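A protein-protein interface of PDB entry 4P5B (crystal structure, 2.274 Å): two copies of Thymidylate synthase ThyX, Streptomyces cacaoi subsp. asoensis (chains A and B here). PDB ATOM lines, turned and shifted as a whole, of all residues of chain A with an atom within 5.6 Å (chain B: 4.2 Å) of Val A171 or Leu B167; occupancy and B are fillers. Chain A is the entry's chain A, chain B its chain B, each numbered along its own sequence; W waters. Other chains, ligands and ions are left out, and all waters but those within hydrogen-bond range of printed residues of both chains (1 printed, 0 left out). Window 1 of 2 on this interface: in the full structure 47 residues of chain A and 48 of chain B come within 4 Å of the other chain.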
ATOM      1  N   PRO A  77      30.209  26.255 -24.745  1.00  0.00           N
ATOM      2  CA  PRO A  77      30.117  25.340 -23.595  1.00  0.00           C
ATOM      3  C   PRO A  77      30.149  23.913 -24.096  1.00  0.00           C
ATOM      4  O   PRO A  77      29.844  23.648 -25.272  1.00  0.00           O
ATOM      5  CB  PRO A  77      28.721  25.644 -23.034  1.00  0.00           C
ATOM      6  CG  PRO A  77      27.978  26.264 -24.185  1.00  0.00           C
ATOM      7  CD  PRO A  77      29.052  27.150 -24.787  1.00  0.00           C
ATOM      8  N   ILE A  78      30.517  23.000 -23.217  1.00  0.00           N
ATOM      9  CA  ILE A  78      30.677  21.644 -23.595  1.00  0.00           C
ATOM     10  C   ILE A  78      29.460  21.019 -24.259  1.00  0.00           C
ATOM     11  O   ILE A  78      29.614  20.273 -25.238  1.00  0.00           O
ATOM     12  CB  ILE A  78      31.099  20.850 -22.386  1.00  0.00           C
ATOM     13  CG1 ILE A  78      32.568  21.128 -22.076  1.00  0.00           C
ATOM     14  CG2 ILE A  78      30.860  19.297 -22.563  1.00  0.00           C
ATOM     15  CD1 ILE A  78      33.029  20.534 -20.675  1.00  0.00           C
ATOM     16  N   PHE A  79      28.254  21.342 -23.789  1.00  0.00           N
ATOM     17  CA  PHE A  79      27.046  20.720 -24.374  1.00  0.00           C
ATOM     18  C   PHE A  79      26.862  21.097 -25.880  1.00  0.00           C
ATOM     19  O   PHE A  79      26.406  20.300 -26.647  1.00  0.00           O
ATOM     20  CB  PHE A  79      25.772  20.969 -23.535  1.00  0.00           C
ATOM     21  CG  PHE A  79      25.222  22.386 -23.686  1.00  0.00           C
ATOM     22  CD1 PHE A  79      25.560  23.392 -22.779  1.00  0.00           C
ATOM     23  CD2 PHE A  79      24.402  22.701 -24.743  1.00  0.00           C
ATOM     24  CE1 PHE A  79      25.106  24.712 -22.942  1.00  0.00           C
ATOM     25  CE2 PHE A  79      23.927  24.021 -24.889  1.00  0.00           C
ATOM     26  CZ  PHE A  79      24.309  25.033 -23.963  1.00  0.00           C
ATOM     27  N   THR A  80      27.326  22.267 -26.292  1.00  0.00           N
ATOM     28  CA  THR A  80      27.252  22.656 -27.662  1.00  0.00           C
ATOM     29  C   THR A  80      28.406  22.047 -28.435  1.00  0.00           C
ATOM     30  O   THR A  80      28.234  21.698 -29.613  1.00  0.00           O
ATOM     31  CB  THR A  80      27.344  24.188 -27.770  1.00  0.00           C
ATOM     32  OG1 THR A  80      26.217  24.745 -27.115  1.00  0.00           O
ATOM     33  CG2 THR A  80      27.349  24.684 -29.241  1.00  0.00           C
ATOM     34  N   TYR A 107      28.337  28.984 -19.389  1.00  0.00           N
ATOM     35  CA  TYR A 107      27.334  29.514 -20.219  1.00  0.00           C
ATOM     36  C   TYR A 107      26.015  29.651 -19.482  1.00  0.00           C
ATOM     37  O   TYR A 107      25.584  28.727 -18.830  1.00  0.00           O
ATOM     38  CB  TYR A 107      27.146  28.612 -21.438  1.00  0.00           C
ATOM     39  CG  TYR A 107      26.077  29.098 -22.380  1.00  0.00           C
ATOM     40  CD1 TYR A 107      24.817  28.586 -22.297  1.00  0.00           C
ATOM     41  CD2 TYR A 107      26.311  30.130 -23.282  1.00  0.00           C
ATOM     42  CE1 TYR A 107      23.800  29.026 -23.108  1.00  0.00           C
ATOM     43  CE2 TYR A 107      25.264  30.603 -24.113  1.00  0.00           C
ATOM     44  CZ  TYR A 107      24.047  30.040 -24.033  1.00  0.00           C
ATOM     45  OH  TYR A 107      22.993  30.454 -24.840  1.00  0.00           O
ATOM     46  N   VAL A 108      25.367  30.799 -19.627  1.00  0.00           N
ATOM     47  CA  VAL A 108      23.921  30.948 -19.396  1.00  0.00           C
ATOM     48  C   VAL A 108      23.306  31.643 -20.587  1.00  0.00           C
ATOM     49  O   VAL A 108      23.935  32.531 -21.170  1.00  0.00           O
ATOM     50  CB  VAL A 108      23.581  31.851 -18.198  1.00  0.00           C
ATOM     51  CG1 VAL A 108      24.059  31.196 -16.971  1.00  0.00           C
ATOM     52  CG2 VAL A 108      24.224  33.285 -18.416  1.00  0.00           C
ATOM     53  N   PRO A 109      22.086  31.235 -20.977  1.00  0.00           N
ATOM     54  CA  PRO A 109      21.411  31.844 -22.125  1.00  0.00           C
ATOM     55  C   PRO A 109      21.168  33.335 -21.870  1.00  0.00           C
ATOM     56  O   PRO A 109      21.046  33.770 -20.705  1.00  0.00           O
ATOM     57  CB  PRO A 109      20.067  31.149 -22.175  1.00  0.00           C
ATOM     58  CG  PRO A 109      20.060  30.136 -21.091  1.00  0.00           C
ATOM     59  CD  PRO A 109      21.290  30.206 -20.282  1.00  0.00           C
ATOM     60  N   TYR A 145      26.826  26.360 -10.562  1.00  0.00           N
ATOM     61  CA  TYR A 145      28.179  26.558 -11.090  1.00  0.00           C
ATOM     62  C   TYR A 145      29.140  26.947 -10.018  1.00  0.00           C
ATOM     63  O   TYR A 145      30.286  26.441  -9.984  1.00  0.00           O
ATOM     64  CB  TYR A 145      28.203  27.698 -12.114  1.00  0.00           C
ATOM     65  CG  TYR A 145      27.352  27.532 -13.317  1.00  0.00           C
ATOM     66  CD1 TYR A 145      26.832  26.286 -13.647  1.00  0.00           C
ATOM     67  CD2 TYR A 145      27.097  28.628 -14.170  1.00  0.00           C
ATOM     68  CE1 TYR A 145      26.009  26.131 -14.750  1.00  0.00           C
ATOM     69  CE2 TYR A 145      26.274  28.497 -15.289  1.00  0.00           C
ATOM     70  CZ  TYR A 145      25.744  27.230 -15.582  1.00  0.00           C
ATOM     71  OH  TYR A 145      24.923  27.071 -16.707  1.00  0.00           O
ATOM     72  N   LEU A 169      32.225  19.480 -12.859  1.00  0.00           N
ATOM     73  CA  LEU A 169      31.958  20.697 -13.665  1.00  0.00           C
ATOM     74  C   LEU A 169      30.769  20.477 -14.572  1.00  0.00           C
ATOM     75  O   LEU A 169      30.619  19.399 -15.149  1.00  0.00           O
ATOM     76  CB  LEU A 169      33.198  21.103 -14.464  1.00  0.00           C
ATOM     77  CG  LEU A 169      34.408  21.490 -13.596  1.00  0.00           C
ATOM     78  CD1 LEU A 169      35.609  21.739 -14.524  1.00  0.00           C
ATOM     79  CD2 LEU A 169      34.113  22.726 -12.734  1.00  0.00           C
ATOM     80  N   PRO A 170      29.912  21.485 -14.705  1.00  0.00           N
ATOM     81  CA  PRO A 170      28.710  21.281 -15.510  1.00  0.00           C
ATOM     82  C   PRO A 170      29.018  21.248 -17.016  1.00  0.00           C
ATOM     83  O   PRO A 170      30.077  21.678 -17.423  1.00  0.00           O
ATOM     84  CB  PRO A 170      27.899  22.547 -15.203  1.00  0.00           C
ATOM     85  CG  PRO A 170      28.948  23.592 -14.921  1.00  0.00           C
ATOM     86  CD  PRO A 170      30.019  22.866 -14.186  1.00  0.00           C
ATOM     87  N   VAL A 171      28.079  20.806 -17.833  1.00  0.00           N
ATOM     88  CA  VAL A 171      28.271  20.799 -19.293  1.00  0.00           C
ATOM     89  C   VAL A 171      28.205  22.208 -19.926  1.00  0.00           C
ATOM     90  O   VAL A 171      28.422  22.379 -21.153  1.00  0.00           O
ATOM     91  CB  VAL A 171      27.249  19.842 -19.956  1.00  0.00           C
ATOM     92  CG1 VAL A 171      27.498  18.391 -19.509  1.00  0.00           C
ATOM     93  CG2 VAL A 171      25.819  20.238 -19.596  1.00  0.00           C
ATOM     94  N   SER A 172      27.953  23.218 -19.092  1.00  0.00           N
ATOM     95  CA  SER A 172      27.932  24.574 -19.561  1.00  0.00           C
ATOM     96  C   SER A 172      29.297  25.227 -19.426  1.00  0.00           C
ATOM     97  O   SER A 172      29.453  26.417 -19.764  1.00  0.00           O
ATOM     98  CB  SER A 172      26.898  25.393 -18.758  1.00  0.00           C
ATOM     99  OG  SER A 172      27.449  25.478 -17.433  1.00  0.00           O
ATOM    100  N   THR A 173      30.275  24.508 -18.886  1.00  0.00           N
ATOM    101  CA  THR A 173      31.646  25.020 -18.830  1.00  0.00           C
ATOM    102  C   THR A 173      32.112  25.379 -20.238  1.00  0.00           C
ATOM    103  O   THR A 173      31.943  24.607 -21.162  1.00  0.00           O
ATOM    104  CB  THR A 173      32.604  23.962 -18.209  1.00  0.00           C
ATOM    105  OG1 THR A 173      32.060  23.558 -16.931  1.00  0.00           O
ATOM    106  CG2 THR A 173      34.054  24.522 -17.965  1.00  0.00           C
ATOM    107  N   GLN A 206      19.439  22.665 -31.271  1.00  0.00           N
ATOM    108  CA  GLN A 206      19.465  23.568 -30.084  1.00  0.00           C
ATOM    109  C   GLN A 206      19.957  24.959 -30.533  1.00  0.00           C
ATOM    110  O   GLN A 206      20.779  25.065 -31.440  1.00  0.00           O
ATOM    111  CB  GLN A 206      20.443  23.063 -29.008  1.00  0.00           C
ATOM    112  CG  GLN A 206      20.339  23.862 -27.741  1.00  0.00           C
ATOM    113  CD  GLN A 206      20.520  23.034 -26.500  1.00  0.00           C
ATOM    114  OE1 GLN A 206      20.521  21.794 -26.551  1.00  0.00           O
ATOM    115  NE2 GLN A 206      20.710  23.701 -25.369  1.00  0.00           N
ATOM    116  N   GLU B 163      16.433  21.092 -22.473  1.00  0.00           N
ATOM    117  CA  GLU B 163      17.714  21.346 -23.091  1.00  0.00           C
ATOM    118  C   GLU B 163      18.396  22.540 -22.433  1.00  0.00           C
ATOM    119  O   GLU B 163      19.577  22.744 -22.650  1.00  0.00           O
ATOM    120  CB  GLU B 163      17.529  21.640 -24.585  1.00  0.00           C
ATOM    121  CG  GLU B 163      17.009  23.028 -24.879  1.00  0.00           C
ATOM    122  CD  GLU B 163      16.850  23.323 -26.349  1.00  0.00           C
ATOM    123  OE1 GLU B 163      16.617  24.492 -26.726  1.00  0.00           O
ATOM    124  OE2 GLU B 163      16.958  22.404 -27.161  1.00  0.00           O
ATOM    125  N   ILE B 164      17.641  23.357 -21.674  1.00  0.00           N
ATOM    126  CA  ILE B 164      18.248  24.450 -20.959  1.00  0.00           C
ATOM    127  C   ILE B 164      18.512  23.993 -19.573  1.00  0.00           C
ATOM    128  O   ILE B 164      19.581  24.291 -19.012  1.00  0.00           O
ATOM    129  CB  ILE B 164      17.355  25.733 -20.933  1.00  0.00           C
ATOM    130  CG1 ILE B 164      17.224  26.334 -22.330  1.00  0.00           C
ATOM    131  CG2 ILE B 164      17.969  26.823 -19.980  1.00  0.00           C
ATOM    132  CD1 ILE B 164      18.544  26.931 -22.834  1.00  0.00           C
ATOM    133  N   ALA B 165      17.593  23.249 -18.995  1.00  0.00           N
ATOM    134  CA  ALA B 165      17.728  22.908 -17.555  1.00  0.00           C
ATOM    135  C   ALA B 165      19.000  22.114 -17.342  1.00  0.00           C
ATOM    136  O   ALA B 165      19.717  22.300 -16.376  1.00  0.00           O
ATOM    137  CB  ALA B 165      16.537  22.088 -17.058  1.00  0.00           C
ATOM    138  N   ARG B 166      19.321  21.264 -18.291  1.00  0.00           N
ATOM    139  CA  ARG B 166      20.478  20.395 -18.150  1.00  0.00           C
ATOM    140  C   ARG B 166      21.796  21.147 -18.135  1.00  0.00           C
ATOM    141  O   ARG B 166      22.840  20.515 -17.925  1.00  0.00           O
ATOM    142  CB  ARG B 166      20.460  19.345 -19.243  1.00  0.00           C
ATOM    143  CG  ARG B 166      20.515  19.900 -20.706  1.00  0.00           C
ATOM    144  CD  ARG B 166      21.944  20.207 -21.284  1.00  0.00           C
ATOM    145  NE  ARG B 166      21.735  20.503 -22.707  1.00  0.00           N
ATOM    146  CZ  ARG B 166      21.920  19.614 -23.679  1.00  0.00           C
ATOM    147  NH1 ARG B 166      22.435  18.406 -23.400  1.00  0.00           N
ATOM    148  NH2 ARG B 166      21.603  19.925 -24.924  1.00  0.00           N
ATOM    149  N   LEU B 167      21.788  22.480 -18.387  1.00  0.00           N
ATOM    150  CA  LEU B 167      23.074  23.155 -18.393  1.00  0.00           C
ATOM    151  C   LEU B 167      23.743  23.027 -17.050  1.00  0.00           C
ATOM    152  O   LEU B 167      24.975  23.065 -16.976  1.00  0.00           O
ATOM    153  CB  LEU B 167      22.986  24.628 -18.744  1.00  0.00           C
ATOM    154  CG  LEU B 167      22.327  25.051 -20.050  1.00  0.00           C
ATOM    155  CD1 LEU B 167      22.488  26.562 -20.324  1.00  0.00           C
ATOM    156  CD2 LEU B 167      22.740  24.213 -21.145  1.00  0.00           C
ATOM    157  N   VAL B 168      22.952  22.902 -15.969  1.00  0.00           N
ATOM    158  CA  VAL B 168      23.552  22.727 -14.652  1.00  0.00           C
ATOM    159  C   VAL B 168      24.138  21.331 -14.354  1.00  0.00           C
ATOM    160  O   VAL B 168      24.794  21.167 -13.358  1.00  0.00           O
ATOM    161  CB  VAL B 168      22.528  23.096 -13.535  1.00  0.00           C
ATOM    162  CG1 VAL B 168      22.023  24.467 -13.745  1.00  0.00           C
ATOM    163  CG2 VAL B 168      21.315  22.083 -13.499  1.00  0.00           C
ATOM    164  N   LEU B 169      23.860  20.300 -15.138  1.00  0.00           N
ATOM    165  CA  LEU B 169      24.365  18.940 -14.799  1.00  0.00           C
ATOM    166  C   LEU B 169      25.873  18.677 -15.100  1.00  0.00           C
ATOM    167  O   LEU B 169      26.401  19.124 -16.137  1.00  0.00           O
ATOM    168  CB  LEU B 169      23.502  17.879 -15.507  1.00  0.00           C
ATOM    169  CG  LEU B 169      22.029  17.963 -15.124  1.00  0.00           C
ATOM    170  CD1 LEU B 169      21.212  17.005 -15.927  1.00  0.00           C
ATOM    171  CD2 LEU B 169      21.862  17.713 -13.558  1.00  0.00           C
ATOM    172  N   VAL B 171      29.620  16.776 -15.875  1.00  0.00           N
ATOM    173  CA  VAL B 171      30.044  15.855 -16.966  1.00  0.00           C
ATOM    174  C   VAL B 171      30.202  14.431 -16.434  1.00  0.00           C
ATOM    175  O   VAL B 171      30.584  13.463 -17.191  1.00  0.00           O
ATOM    176  CB  VAL B 171      31.357  16.278 -17.620  1.00  0.00           C
ATOM    177  CG1 VAL B 171      31.241  17.674 -18.321  1.00  0.00           C
ATOM    178  CG2 VAL B 171      32.466  16.295 -16.639  1.00  0.00           C
HETATM  179  O   HOH W   1      24.999  18.039 -25.566  1.00  0.00           O
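Water W1 lies within hydrogen-bond range of the backbone carbonyl oxygen of Phe A79 (2.9 Å) and the guanidinium group of Arg B166 (3.4 Å).
Among the printed residues, pairs that only touch across the chains: Phe A79 with Arg B166, Phe A79 with Leu B167, Tyr A107 with Leu B167, Pro A109 with Ile B164, Pro A109 with Leu B167, Tyr A145 with Leu B167, Pro A170 with Leu B167, Pro A170 with Val B168, Pro A170 with Leu B169, Val A171 with Arg B166, Val A171 with Leu B167 and Val A171 with Val B171.
Printed residues of chain B that touch a printed residue of chain A: Glu B163, Ile B164, Arg B166, Leu B167, Val B168, Leu B169 and Val B171. Hydrophobic or aromatic side chains of chain B that line the printed part of chain A: Ile B164, Leu B167 and Val B171. Among the printed residues, 17 pairs touch across the chains. Among the printed residues, no Asp or Glu carboxylate lies within 4 Å of a Lys or Arg side-chain nitrogen of the other chain.
The backbone NH (N) of Val A171 sits at hydrogen-bond distance from the backbone carbonyl oxygen (O) of Leu B169, at 2.9 Å. NE2 of Gln A206 is in hydrogen-bond range of O of Glu B163. OE1 of Gln A206 is in hydrogen-bond range of NH2 of Arg B166 (2.7 Å). OG of Ser A172 is in hydrogen-bond range of O of Leu B167 (3.5 Å). The backbone NH (N) of Val B171 is in hydrogen-bond range of the backbone carbonyl oxygen (O) of Leu A169.
Printed residues of chain B within 4 Å of Tyr A107: Leu B167. Printed residues of chain B within 4 Å of Ser A172: Leu B167. Of the printed residues of chain A, Glu B163 touches Gln A206 (3.1 Å). Printed residues of chain A within 4 Å of Ile B164: Pro A109. Leu B167 touches just these residues of chain A: Phe A79, Tyr A107, Pro A109, Tyr A145, Pro A170, Val A171 and Ser A172. The nearest printed residue of chain B that does not touch Val A171 is Val B168 (5.3 Å). The nearest printed residue of chain B that does not touch Gln A206 is Ile B164 (4.6 Å).
The backbone carbonyl oxygen of Val A171 is in hydrogen-bond range of the backbone NH of Phe A79 (2.8 Å). The backbone NH (N) of Ile A78 lies within hydrogen-bond range of the backbone carbonyl oxygen (O) of Val A171, 3.0 Å away. O of Ser A172 is in hydrogen-bond range of N of Tyr A107, at 2.8 Å. The backbone carbonyl oxygen (O) of Glu B163 sits at hydrogen-bond distance from the guanidinium group (NE) of Arg B166, at 3.1 Å. O of Tyr A107 is in hydrogen-bond range of OH of Tyr A145 (2.8 Å). O of Pro A170 lies within hydrogen-bond range of OG1 of Thr A173, 2.8 Å away.
Leu A169 touches Val B171, and with the chains exchanged Val A171 touches Leu B169. Val A171 touches its own counterpart, Val B171. Positions printed for both chains: 169 and 171.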
